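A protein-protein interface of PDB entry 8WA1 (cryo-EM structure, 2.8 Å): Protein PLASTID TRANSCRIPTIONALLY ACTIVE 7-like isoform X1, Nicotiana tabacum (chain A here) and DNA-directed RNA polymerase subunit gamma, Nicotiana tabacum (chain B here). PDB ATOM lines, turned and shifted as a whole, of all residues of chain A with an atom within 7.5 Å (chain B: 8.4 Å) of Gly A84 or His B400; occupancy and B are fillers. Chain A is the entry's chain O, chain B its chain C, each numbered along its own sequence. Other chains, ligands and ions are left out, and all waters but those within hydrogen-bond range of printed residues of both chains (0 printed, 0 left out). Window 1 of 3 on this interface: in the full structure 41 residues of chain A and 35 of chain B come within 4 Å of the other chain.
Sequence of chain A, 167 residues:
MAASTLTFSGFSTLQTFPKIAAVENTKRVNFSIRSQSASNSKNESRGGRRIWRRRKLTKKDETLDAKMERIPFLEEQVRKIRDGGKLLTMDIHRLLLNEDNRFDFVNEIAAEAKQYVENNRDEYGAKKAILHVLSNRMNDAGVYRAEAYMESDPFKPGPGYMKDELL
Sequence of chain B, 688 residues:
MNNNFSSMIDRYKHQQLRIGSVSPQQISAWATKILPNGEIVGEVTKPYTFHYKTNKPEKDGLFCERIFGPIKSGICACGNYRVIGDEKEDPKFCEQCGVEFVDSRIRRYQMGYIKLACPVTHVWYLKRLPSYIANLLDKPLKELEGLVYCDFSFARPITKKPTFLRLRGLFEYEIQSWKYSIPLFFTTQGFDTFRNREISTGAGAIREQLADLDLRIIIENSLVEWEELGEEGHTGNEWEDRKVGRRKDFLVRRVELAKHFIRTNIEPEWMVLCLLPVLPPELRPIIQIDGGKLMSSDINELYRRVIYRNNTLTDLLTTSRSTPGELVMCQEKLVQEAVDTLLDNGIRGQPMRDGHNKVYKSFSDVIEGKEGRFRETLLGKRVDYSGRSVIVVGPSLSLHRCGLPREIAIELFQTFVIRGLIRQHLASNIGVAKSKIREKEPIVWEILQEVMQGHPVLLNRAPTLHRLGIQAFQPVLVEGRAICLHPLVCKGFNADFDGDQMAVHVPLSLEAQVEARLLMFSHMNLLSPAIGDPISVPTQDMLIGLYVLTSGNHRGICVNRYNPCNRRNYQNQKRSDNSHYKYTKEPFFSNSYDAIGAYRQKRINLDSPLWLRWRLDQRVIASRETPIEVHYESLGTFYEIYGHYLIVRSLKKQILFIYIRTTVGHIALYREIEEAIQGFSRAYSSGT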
ATOM      1  N   VAL A  78     -17.062  30.638 -31.892  1.00  0.00           N
ATOM      2  CA  VAL A  78     -17.620  29.820 -32.966  1.00  0.00           C
ATOM      3  C   VAL A  78     -17.134  28.382 -32.843  1.00  0.00           C
ATOM      4  O   VAL A  78     -17.887  27.430 -33.094  1.00  0.00           O
ATOM      5  CB  VAL A  78     -17.269  30.425 -34.339  1.00  0.00           C
ATOM      6  CG1 VAL A  78     -17.805  29.551 -35.461  1.00  0.00           C
ATOM      7  CG2 VAL A  78     -17.824  31.835 -34.455  1.00  0.00           C
ATOM      8  N   ARG A  79     -15.871  28.199 -32.447  1.00  0.00           N
ATOM      9  CA  ARG A  79     -15.344  26.853 -32.244  1.00  0.00           C
ATOM     10  C   ARG A  79     -16.145  26.106 -31.185  1.00  0.00           C
ATOM     11  O   ARG A  79     -16.508  24.939 -31.368  1.00  0.00           O
ATOM     12  CB  ARG A  79     -13.871  26.927 -31.848  1.00  0.00           C
ATOM     13  CG  ARG A  79     -13.172  25.583 -31.784  1.00  0.00           C
ATOM     14  CD  ARG A  79     -11.952  25.651 -30.882  1.00  0.00           C
ATOM     15  NE  ARG A  79     -11.314  26.965 -30.924  1.00  0.00           N
ATOM     16  CZ  ARG A  79     -10.401  27.328 -31.818  1.00  0.00           C
ATOM     17  NH1 ARG A  79     -10.012  26.476 -32.755  1.00  0.00           N
ATOM     18  NH2 ARG A  79      -9.878  28.545 -31.776  1.00  0.00           N
ATOM     19  N   LYS A  80     -16.441  26.774 -30.066  1.00  0.00           N
ATOM     20  CA  LYS A  80     -17.184  26.130 -28.991  1.00  0.00           C
ATOM     21  C   LYS A  80     -18.633  25.885 -29.393  1.00  0.00           C
ATOM     22  O   LYS A  80     -19.231  24.877 -28.999  1.00  0.00           O
ATOM     23  CB  LYS A  80     -17.113  26.979 -27.723  1.00  0.00           C
ATOM     24  CG  LYS A  80     -17.639  26.286 -26.477  1.00  0.00           C
ATOM     25  CD  LYS A  80     -16.813  25.053 -26.143  1.00  0.00           C
ATOM     26  CE  LYS A  80     -15.361  25.415 -25.871  1.00  0.00           C
ATOM     27  NZ  LYS A  80     -14.531  24.212 -25.583  1.00  0.00           N
ATOM     28  N   ILE A  81     -19.217  26.796 -30.176  1.00  0.00           N
ATOM     29  CA  ILE A  81     -20.578  26.588 -30.666  1.00  0.00           C
ATOM     30  C   ILE A  81     -20.637  25.353 -31.555  1.00  0.00           C
ATOM     31  O   ILE A  81     -21.570  24.546 -31.462  1.00  0.00           O
ATOM     32  CB  ILE A  81     -21.083  27.842 -31.403  1.00  0.00           C
ATOM     33  CG1 ILE A  81     -21.290  28.995 -30.421  1.00  0.00           C
ATOM     34  CG2 ILE A  81     -22.380  27.544 -32.139  1.00  0.00           C
ATOM     35  CD1 ILE A  81     -21.749  30.277 -31.080  1.00  0.00           C
ATOM     36  N   ARG A  82     -19.640  25.180 -32.427  1.00  0.00           N
ATOM     37  CA  ARG A  82     -19.624  24.011 -33.300  1.00  0.00           C
ATOM     38  C   ARG A  82     -19.369  22.733 -32.509  1.00  0.00           C
ATOM     39  O   ARG A  82     -19.990  21.696 -32.768  1.00  0.00           O
ATOM     40  CB  ARG A  82     -18.571  24.179 -34.396  1.00  0.00           C
ATOM     41  CG  ARG A  82     -18.836  25.323 -35.355  1.00  0.00           C
ATOM     42  CD  ARG A  82     -18.007  25.170 -36.621  1.00  0.00           C
ATOM     43  NE  ARG A  82     -16.626  24.794 -36.328  1.00  0.00           N
ATOM     44  CZ  ARG A  82     -15.634  25.661 -36.161  1.00  0.00           C
ATOM     45  NH1 ARG A  82     -15.866  26.963 -36.258  1.00  0.00           N
ATOM     46  NH2 ARG A  82     -14.409  25.230 -35.896  1.00  0.00           N
ATOM     47  N   ASP A  83     -18.452  22.786 -31.540  1.00  0.00           N
ATOM     48  CA  ASP A  83     -18.063  21.577 -30.821  1.00  0.00           C
ATOM     49  C   ASP A  83     -19.152  21.117 -29.858  1.00  0.00           C
ATOM     50  O   ASP A  83     -19.390  19.912 -29.713  1.00  0.00           O
ATOM     51  CB  ASP A  83     -16.752  21.817 -30.073  1.00  0.00           C
ATOM     52  CG  ASP A  83     -16.112  20.532 -29.593  1.00  0.00           C
ATOM     53  OD1 ASP A  83     -16.527  19.449 -30.058  1.00  0.00           O
ATOM     54  OD2 ASP A  83     -15.192  20.603 -28.751  1.00  0.00           O
ATOM     55  N   GLY A  84     -19.818  22.057 -29.184  1.00  0.00           N
ATOM     56  CA  GLY A  84     -20.774  21.678 -28.154  1.00  0.00           C
ATOM     57  C   GLY A  84     -21.990  20.957 -28.702  1.00  0.00           C
ATOM     58  O   GLY A  84     -22.425  19.946 -28.146  1.00  0.00           O
ATOM     59  N   GLY A  85     -22.557  21.464 -29.793  1.00  0.00           N
ATOM     60  CA  GLY A  85     -23.733  20.847 -30.373  1.00  0.00           C
ATOM     61  C   GLY A  85     -24.886  21.808 -30.573  1.00  0.00           C
ATOM     62  O   GLY A  85     -26.012  21.383 -30.847  1.00  0.00           O
ATOM     63  N   LYS A  86     -24.619  23.110 -30.440  1.00  0.00           N
ATOM     64  CA  LYS A  86     -25.662  24.102 -30.682  1.00  0.00           C
ATOM     65  C   LYS A  86     -26.061  24.145 -32.151  1.00  0.00           C
ATOM     66  O   LYS A  86     -27.137  24.656 -32.487  1.00  0.00           O
ATOM     67  CB  LYS A  86     -25.193  25.480 -30.214  1.00  0.00           C
ATOM     68  CG  LYS A  86     -24.725  25.513 -28.771  1.00  0.00           C
ATOM     69  CD  LYS A  86     -24.440  26.935 -28.319  1.00  0.00           C
ATOM     70  CE  LYS A  86     -25.704  27.774 -28.330  1.00  0.00           C
ATOM     71  NZ  LYS A  86     -26.756  27.189 -27.453  1.00  0.00           N
ATOM     72  N   LEU A  87     -25.202  23.629 -33.036  1.00  0.00           N
ATOM     73  CA  LEU A  87     -25.569  23.501 -34.442  1.00  0.00           C
ATOM     74  C   LEU A  87     -26.847  22.688 -34.597  1.00  0.00           C
ATOM     75  O   LEU A  87     -27.685  22.990 -35.455  1.00  0.00           O
ATOM     76  CB  LEU A  87     -24.427  22.852 -35.226  1.00  0.00           C
ATOM     77  CG  LEU A  87     -23.001  23.319 -34.931  1.00  0.00           C
ATOM     78  CD1 LEU A  87     -22.008  22.493 -35.731  1.00  0.00           C
ATOM     79  CD2 LEU A  87     -22.832  24.797 -35.232  1.00  0.00           C
ATOM     80  N   LEU A  88     -27.013  21.656 -33.767  1.00  0.00           N
ATOM     81  CA  LEU A  88     -28.229  20.850 -33.814  1.00  0.00           C
ATOM     82  C   LEU A  88     -29.454  21.686 -33.470  1.00  0.00           C
ATOM     83  O   LEU A  88     -30.494  21.576 -34.130  1.00  0.00           O
ATOM     84  CB  LEU A  88     -28.104  19.662 -32.863  1.00  0.00           C
ATOM     85  CG  LEU A  88     -29.240  18.642 -32.903  1.00  0.00           C
ATOM     86  CD1 LEU A  88     -29.356  18.041 -34.293  1.00  0.00           C
ATOM     87  CD2 LEU A  88     -29.023  17.556 -31.863  1.00  0.00           C
ATOM     88  N   THR A  89     -29.349  22.537 -32.446  1.00  0.00           N
ATOM     89  CA  THR A  89     -30.473  23.391 -32.076  1.00  0.00           C
ATOM     90  C   THR A  89     -30.792  24.392 -33.179  1.00  0.00           C
ATOM     91  O   THR A  89     -31.967  24.634 -33.489  1.00  0.00           O
ATOM     92  CB  THR A  89     -30.170  24.122 -30.769  1.00  0.00           C
ATOM     93  OG1 THR A  89     -29.115  25.066 -30.981  1.00  0.00           O
ATOM     94  CG2 THR A  89     -29.741  23.132 -29.696  1.00  0.00           C
ATOM     95  N   GLU A 165     -15.637  16.739 -19.180  1.00  0.00           N
ATOM     96  CA  GLU A 165     -16.367  17.960 -19.503  1.00  0.00           C
ATOM     97  C   GLU A 165     -17.025  18.482 -18.233  1.00  0.00           C
ATOM     98  O   GLU A 165     -18.012  17.914 -17.756  1.00  0.00           O
ATOM     99  CB  GLU A 165     -17.400  17.704 -20.598  1.00  0.00           C
ATOM    100  CG  GLU A 165     -16.807  17.226 -21.913  1.00  0.00           C
ATOM    101  CD  GLU A 165     -17.855  17.040 -22.993  1.00  0.00           C
ATOM    102  OE1 GLU A 165     -19.005  17.480 -22.787  1.00  0.00           O
ATOM    103  OE2 GLU A 165     -17.528  16.453 -24.046  1.00  0.00           O
ATOM    104  N   LEU B 397     -22.202  24.587 -18.182  1.00  0.00           N
ATOM    105  CA  LEU B 397     -22.899  23.574 -18.917  1.00  0.00           C
ATOM    106  C   LEU B 397     -23.716  24.438 -19.828  1.00  0.00           C
ATOM    107  O   LEU B 397     -23.790  25.631 -19.600  1.00  0.00           O
ATOM    108  CB  LEU B 397     -23.807  22.790 -17.989  1.00  0.00           C
ATOM    109  CG  LEU B 397     -23.275  21.649 -17.142  1.00  0.00           C
ATOM    110  CD1 LEU B 397     -24.407  21.142 -16.269  1.00  0.00           C
ATOM    111  CD2 LEU B 397     -22.768  20.542 -18.046  1.00  0.00           C
ATOM    112  N   SER B 398     -24.279  23.894 -20.890  1.00  0.00           N
ATOM    113  CA  SER B 398     -25.147  24.690 -21.721  1.00  0.00           C
ATOM    114  C   SER B 398     -26.587  24.295 -21.506  1.00  0.00           C
ATOM    115  O   SER B 398     -26.845  23.275 -20.907  1.00  0.00           O
ATOM    116  CB  SER B 398     -24.753  24.514 -23.153  1.00  0.00           C
ATOM    117  OG  SER B 398     -23.348  24.590 -23.284  1.00  0.00           O
ATOM    118  N   LEU B 399     -27.532  25.093 -21.971  1.00  0.00           N
ATOM    119  CA  LEU B 399     -28.946  24.830 -21.728  1.00  0.00           C
ATOM    120  C   LEU B 399     -29.347  23.431 -22.178  1.00  0.00           C
ATOM    121  O   LEU B 399     -30.304  22.860 -21.645  1.00  0.00           O
ATOM    122  CB  LEU B 399     -29.803  25.880 -22.433  1.00  0.00           C
ATOM    123  CG  LEU B 399     -29.670  27.310 -21.908  1.00  0.00           C
ATOM    124  CD1 LEU B 399     -30.472  28.277 -22.761  1.00  0.00           C
ATOM    125  CD2 LEU B 399     -30.109  27.383 -20.455  1.00  0.00           C
ATOM    126  N   HIS B 400     -28.636  22.865 -23.157  1.00  0.00           N
ATOM    127  CA  HIS B 400     -29.006  21.548 -23.662  1.00  0.00           C
ATOM    128  C   HIS B 400     -28.235  20.430 -22.971  1.00  0.00           C
ATOM    129  O   HIS B 400     -28.625  19.262 -23.071  1.00  0.00           O
ATOM    130  CB  HIS B 400     -28.800  21.489 -25.176  1.00  0.00           C
ATOM    131  CG  HIS B 400     -27.399  21.782 -25.613  1.00  0.00           C
ATOM    132  ND1 HIS B 400     -26.957  23.058 -25.888  1.00  0.00           N
ATOM    133  CD2 HIS B 400     -26.344  20.962 -25.835  1.00  0.00           C
ATOM    134  CE1 HIS B 400     -25.688  23.013 -26.254  1.00  0.00           C
ATOM    135  NE2 HIS B 400     -25.292  21.753 -26.230  1.00  0.00           N
ATOM    136  N   ARG B 401     -27.150  20.755 -22.273  1.00  0.00           N
ATOM    137  CA  ARG B 401     -26.314  19.755 -21.618  1.00  0.00           C
ATOM    138  C   ARG B 401     -26.561  19.757 -20.116  1.00  0.00           C
ATOM    139  O   ARG B 401     -26.785  20.813 -19.518  1.00  0.00           O
ATOM    140  CB  ARG B 401     -24.833  20.008 -21.905  1.00  0.00           C
ATOM    141  CG  ARG B 401     -24.394  19.593 -23.295  1.00  0.00           C
ATOM    142  CD  ARG B 401     -22.887  19.694 -23.452  1.00  0.00           C
ATOM    143  NE  ARG B 401     -22.429  19.095 -24.702  1.00  0.00           N
ATOM    144  CZ  ARG B 401     -21.153  18.979 -25.051  1.00  0.00           C
ATOM    145  NH1 ARG B 401     -20.198  19.421 -24.245  1.00  0.00           N
ATOM    146  NH2 ARG B 401     -20.828  18.420 -26.208  1.00  0.00           N
ATOM    147  N   CYS B 402     -26.520  18.568 -19.512  1.00  0.00           N
ATOM    148  CA  CYS B 402     -26.639  18.405 -18.070  1.00  0.00           C
ATOM    149  C   CYS B 402     -25.629  17.367 -17.607  1.00  0.00           C
ATOM    150  O   CYS B 402     -25.373  16.387 -18.314  1.00  0.00           O
ATOM    151  CB  CYS B 402     -28.056  17.982 -17.667  1.00  0.00           C
ATOM    152  SG  CYS B 402     -28.491  16.279 -18.098  1.00  0.00           S
ATOM    153  N   GLY B 403     -25.049  17.588 -16.431  1.00  0.00           N
ATOM    154  CA  GLY B 403     -24.113  16.622 -15.883  1.00  0.00           C
ATOM    155  C   GLY B 403     -24.833  15.403 -15.330  1.00  0.00           C
ATOM    156  O   GLY B 403     -25.815  15.514 -14.595  1.00  0.00           O
ATOM    157  N   GLN B 453     -23.961   9.933 -26.797  1.00  0.00           N
ATOM    158  CA  GLN B 453     -23.628  11.225 -27.387  1.00  0.00           C
ATOM    159  C   GLN B 453     -24.831  11.865 -28.068  1.00  0.00           C
ATOM    160  O   GLN B 453     -24.910  13.096 -28.152  1.00  0.00           O
ATOM    161  CB  GLN B 453     -22.478  11.074 -28.382  1.00  0.00           C
ATOM    162  CG  GLN B 453     -21.106  10.987 -27.736  1.00  0.00           C
ATOM    163  CD  GLN B 453     -19.991  10.873 -28.755  1.00  0.00           C
ATOM    164  OE1 GLN B 453     -18.811  10.918 -28.409  1.00  0.00           O
ATOM    165  NE2 GLN B 453     -20.361  10.723 -30.022  1.00  0.00           N
ATOM    166  N   HIS B 455     -28.165  10.673 -27.319  1.00  0.00           N
ATOM    167  CA  HIS B 455     -29.359  10.208 -26.635  1.00  0.00           C
ATOM    168  C   HIS B 455     -29.866  11.263 -25.659  1.00  0.00           C
ATOM    169  O   HIS B 455     -29.082  11.862 -24.919  1.00  0.00           O
ATOM    170  CB  HIS B 455     -29.074   8.911 -25.874  1.00  0.00           C
ATOM    171  CG  HIS B 455     -30.246   7.982 -25.809  1.00  0.00           C
ATOM    172  ND1 HIS B 455     -30.474   7.007 -26.754  1.00  0.00           N
ATOM    173  CD2 HIS B 455     -31.259   7.884 -24.914  1.00  0.00           C
ATOM    174  CE1 HIS B 455     -31.573   6.345 -26.446  1.00  0.00           C
ATOM    175  NE2 HIS B 455     -32.069   6.857 -25.334  1.00  0.00           N
ATOM    176  N   PRO B 456     -31.175  11.514 -25.634  1.00  0.00           N
ATOM    177  CA  PRO B 456     -31.714  12.529 -24.720  1.00  0.00           C
ATOM    178  C   PRO B 456     -32.131  11.957 -23.373  1.00  0.00           C
ATOM    179  O   PRO B 456     -32.624  10.828 -23.291  1.00  0.00           O
ATOM    180  CB  PRO B 456     -32.916  13.085 -25.494  1.00  0.00           C
ATOM    181  CG  PRO B 456     -33.287  12.003 -26.502  1.00  0.00           C
ATOM    182  CD  PRO B 456     -32.224  10.931 -26.485  1.00  0.00           C
ATOM    183  N   VAL B 457     -31.925  12.731 -22.309  1.00  0.00           N
ATOM    184  CA  VAL B 457     -32.280  12.336 -20.950  1.00  0.00           C
ATOM    185  C   VAL B 457     -33.442  13.201 -20.477  1.00  0.00           C
ATOM    186  O   VAL B 457     -33.437  14.423 -20.677  1.00  0.00           O
ATOM    187  CB  VAL B 457     -31.070  12.457 -20.006  1.00  0.00           C
ATOM    188  CG1 VAL B 457     -31.501  12.910 -18.621  1.00  0.00           C
ATOM    189  CG2 VAL B 457     -30.332  11.131 -19.923  1.00  0.00           C
ATOM    190  N   GLN B 471     -38.167  18.269 -18.260  1.00  0.00           N
ATOM    191  CA  GLN B 471     -37.510  18.770 -19.461  1.00  0.00           C
ATOM    192  C   GLN B 471     -36.563  17.723 -20.028  1.00  0.00           C
ATOM    193  O   GLN B 471     -36.514  16.590 -19.538  1.00  0.00           O
ATOM    194  CB  GLN B 471     -36.761  20.071 -19.167  1.00  0.00           C
ATOM    195  CG  GLN B 471     -37.669  21.243 -18.840  1.00  0.00           C
ATOM    196  CD  GLN B 471     -36.907  22.545 -18.703  1.00  0.00           C
ATOM    197  OE1 GLN B 471     -37.444  23.547 -18.230  1.00  0.00           O
ATOM    198  NE2 GLN B 471     -35.647  22.537 -19.118  1.00  0.00           N
ATOM    199  N   ALA B 472     -35.803  18.090 -21.056  1.00  0.00           N
ATOM    200  CA  ALA B 472     -34.893  17.160 -21.704  1.00  0.00           C
ATOM    201  C   ALA B 472     -33.549  17.840 -21.904  1.00  0.00           C
ATOM    202  O   ALA B 472     -33.489  19.019 -22.262  1.00  0.00           O
ATOM    203  CB  ALA B 472     -35.447  16.671 -23.046  1.00  0.00           C
ATOM    204  N   PHE B 473     -32.477  17.087 -21.676  1.00  0.00           N
ATOM    205  CA  PHE B 473     -31.124  17.606 -21.795  1.00  0.00           C
ATOM    206  C   PHE B 473     -30.246  16.553 -22.453  1.00  0.00           C
ATOM    207  O   PHE B 473     -30.684  15.438 -22.746  1.00  0.00           O
ATOM    208  CB  PHE B 473     -30.548  17.999 -20.429  1.00  0.00           C
ATOM    209  CG  PHE B 473     -31.384  18.992 -19.675  1.00  0.00           C
ATOM    210  CD1 PHE B 473     -31.220  20.351 -19.878  1.00  0.00           C
ATOM    211  CD2 PHE B 473     -32.328  18.567 -18.754  1.00  0.00           C
ATOM    212  CE1 PHE B 473     -31.984  21.267 -19.181  1.00  0.00           C
ATOM    213  CE2 PHE B 473     -33.096  19.478 -18.054  1.00  0.00           C
ATOM    214  CZ  PHE B 473     -32.924  20.831 -18.270  1.00  0.00           C
ATOM    215  N   GLN B 474     -28.988  16.922 -22.685  1.00  0.00           N
ATOM    216  CA  GLN B 474     -27.996  16.006 -23.227  1.00  0.00           C
ATOM    217  C   GLN B 474     -27.082  15.554 -22.101  1.00  0.00           C
ATOM    218  O   GLN B 474     -26.347  16.383 -21.542  1.00  0.00           O
ATOM    219  CB  GLN B 474     -27.188  16.672 -24.339  1.00  0.00           C
ATOM    220  CG  GLN B 474     -26.887  15.767 -25.525  1.00  0.00           C
ATOM    221  CD  GLN B 474     -26.041  14.565 -25.154  1.00  0.00           C
ATOM    222  OE1 GLN B 474     -26.270  13.459 -25.641  1.00  0.00           O
ATOM    223  NE2 GLN B 474     -25.051  14.777 -24.295  1.00  0.00           N
ATOM    224  N   PRO B 475     -27.092  14.275 -21.731  1.00  0.00           N
ATOM    225  CA  PRO B 475     -26.275  13.828 -20.594  1.00  0.00           C
ATOM    226  C   PRO B 475     -24.790  13.886 -20.920  1.00  0.00           C
ATOM    227  O   PRO B 475     -24.351  13.434 -21.980  1.00  0.00           O
ATOM    228  CB  PRO B 475     -26.746  12.389 -20.365  1.00  0.00           C
ATOM    229  CG  PRO B 475     -27.256  11.953 -21.698  1.00  0.00           C
ATOM    230  CD  PRO B 475     -27.875  13.175 -22.314  1.00  0.00           C
ATOM    231  N   VAL B 476     -24.020  14.452 -19.995  1.00  0.00           N
ATOM    232  CA  VAL B 476     -22.568  14.507 -20.092  1.00  0.00           C
ATOM    233  C   VAL B 476     -21.991  13.698 -18.940  1.00  0.00           C
ATOM    234  O   VAL B 476     -22.372  13.901 -17.781  1.00  0.00           O
ATOM    235  CB  VAL B 476     -22.048  15.956 -20.061  1.00  0.00           C
ATOM    236  CG1 VAL B 476     -20.533  15.972 -20.134  1.00  0.00           C
ATOM    237  CG2 VAL B 476     -22.650  16.754 -21.205  1.00  0.00           C
ATOM    238  N   HIS B 486     -27.939  23.120 -15.107  1.00  0.00           N
ATOM    239  CA  HIS B 486     -27.615  24.470 -15.531  1.00  0.00           C
ATOM    240  C   HIS B 486     -28.245  25.469 -14.613  1.00  0.00           C
ATOM    241  O   HIS B 486     -29.363  25.293 -14.182  1.00  0.00           O
ATOM    242  CB  HIS B 486     -28.142  24.696 -16.929  1.00  0.00           C
ATOM    243  CG  HIS B 486     -27.561  25.883 -17.615  1.00  0.00           C
ATOM    244  ND1 HIS B 486     -28.134  27.132 -17.556  1.00  0.00           N
ATOM    245  CD2 HIS B 486     -26.462  26.009 -18.387  1.00  0.00           C
ATOM    246  CE1 HIS B 486     -27.406  27.978 -18.258  1.00  0.00           C
ATOM    247  NE2 HIS B 486     -26.385  27.321 -18.775  1.00  0.00           N
ATOM    248  N   VAL B 489     -31.826  27.275 -15.698  1.00  0.00           N
ATOM    249  CA  VAL B 489     -32.999  26.405 -15.794  1.00  0.00           C
ATOM    250  C   VAL B 489     -33.593  26.079 -14.433  1.00  0.00           C
ATOM    251  O   VAL B 489     -34.592  25.353 -14.360  1.00  0.00           O
ATOM    252  CB  VAL B 489     -32.625  25.118 -16.556  1.00  0.00           C
ATOM    253  CG1 VAL B 489     -31.929  24.125 -15.638  1.00  0.00           C
ATOM    254  CG2 VAL B 489     -33.851  24.505 -17.221  1.00  0.00           C
ATOM    255  N   ARG B 517     -35.983  15.140 -28.201  1.00  0.00           N
ATOM    256  CA  ARG B 517     -34.964  16.024 -28.755  1.00  0.00           C
ATOM    257  C   ARG B 517     -35.567  17.282 -29.367  1.00  0.00           C
ATOM    258  O   ARG B 517     -34.930  18.342 -29.346  1.00  0.00           O
ATOM    259  CB  ARG B 517     -34.132  15.275 -29.796  1.00  0.00           C
ATOM    260  CG  ARG B 517     -32.920  16.041 -30.298  1.00  0.00           C
ATOM    261  CD  ARG B 517     -32.076  15.201 -31.246  1.00  0.00           C
ATOM    262  NE  ARG B 517     -31.503  14.028 -30.590  1.00  0.00           N
ATOM    263  CZ  ARG B 517     -32.005  12.800 -30.679  1.00  0.00           C
ATOM    264  NH1 ARG B 517     -33.095  12.579 -31.400  1.00  0.00           N
ATOM    265  NH2 ARG B 517     -31.418  11.794 -30.047  1.00  0.00           N
ATOM    266  N   PHE B 521     -37.000  20.084 -25.273  1.00  0.00           N
ATOM    267  CA  PHE B 521     -35.719  20.688 -24.942  1.00  0.00           C
ATOM    268  C   PHE B 521     -35.911  22.090 -24.361  1.00  0.00           C
ATOM    269  O   PHE B 521     -36.970  22.711 -24.486  1.00  0.00           O
ATOM    270  CB  PHE B 521     -34.812  20.727 -26.169  1.00  0.00           C
ATOM    271  CG  PHE B 521     -33.670  19.756 -26.099  1.00  0.00           C
ATOM    272  CD1 PHE B 521     -33.888  18.399 -26.263  1.00  0.00           C
ATOM    273  CD2 PHE B 521     -32.381  20.196 -25.859  1.00  0.00           C
ATOM    274  CE1 PHE B 521     -32.842  17.501 -26.194  1.00  0.00           C
ATOM    275  CE2 PHE B 521     -31.332  19.301 -25.791  1.00  0.00           C
ATOM    276  CZ  PHE B 521     -31.563  17.953 -25.959  1.00  0.00           C
ATOM    277  N   SER B 522     -34.855  22.584 -23.711  1.00  0.00           N
ATOM    278  CA  SER B 522     -34.944  23.854 -22.997  1.00  0.00           C
ATOM    279  C   SER B 522     -34.970  25.040 -23.952  1.00  0.00           C
ATOM    280  O   SER B 522     -35.706  26.008 -23.724  1.00  0.00           O
ATOM    281  CB  SER B 522     -33.779  23.986 -22.015  1.00  0.00           C
ATOM    282  OG  SER B 522     -33.854  23.000 -21.002  1.00  0.00           O
ATOM    283  N   HIS B 523     -34.169  24.995 -25.020  1.00  0.00           N
ATOM    284  CA  HIS B 523     -34.108  26.118 -25.948  1.00  0.00           C
ATOM    285  C   HIS B 523     -35.431  26.349 -26.666  1.00  0.00           C
ATOM    286  O   HIS B 523     -35.648  27.442 -27.201  1.00  0.00           O
ATOM    287  CB  HIS B 523     -32.988  25.905 -26.970  1.00  0.00           C
ATOM    288  CG  HIS B 523     -33.162  24.684 -27.817  1.00  0.00           C
ATOM    289  ND1 HIS B 523     -32.633  23.459 -27.474  1.00  0.00           N
ATOM    290  CD2 HIS B 523     -33.801  24.500 -28.997  1.00  0.00           C
ATOM    291  CE1 HIS B 523     -32.940  22.572 -28.404  1.00  0.00           C
ATOM    292  NE2 HIS B 523     -33.649  23.178 -29.339  1.00  0.00           N
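Printed residues of chain B that touch a printed residue of chain A: His B400, Arg B401, Val B476, Arg B517 and His B523. Hydrophobic or aromatic side chains of chain B that line the printed part of chain A: His B400, Val B476 and His B523. Among the printed residues, 7 pairs touch across the chains.
The backbone carbonyl oxygen of Lys A86 lies within hydrogen-bond range of the side-chain hydroxyl of Thr A89, 2.5 Å away. N of Val B476 is in hydrogen-bond range of O of Cys B402 (2.9 Å).
Gly A84 touches just these residues of chain B: His B400 and Arg B401. His B400 touches just these residues of chain A: Gly A84 (3.9 Å) and Lys A86 (3.7 Å). Printed residues of chain B within 4 Å of Lys A86: His B400. Of the printed residues of chain A, His B523 touches Thr A89. Printed residues of chain B within 4 Å of Thr A89: His B523. Printed residues of chain A within 4 Å of Arg B517: Leu A88. Printed residues of chain B within 4 Å of Glu A165: Arg B401 and Val B476. The nearest printed residue of chain A that does not touch Arg B401 is Asp A83 (4.1 Å).
The guanidinium group of Arg B401 lies within hydrogen-bond range of the backbone carbonyl oxygen of Gly A84 (2.9 Å). NH1 of Arg B401 is in salt-bridge range of OE1 of Glu A165 (2.7 Å).
Among the printed residues, pairs that only touch across the chains: Glu A165 with Val B476, Thr A89 with His B523, Lys A86 with His B400, Gly A84 with His B400 and Leu A88 with Arg B517.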
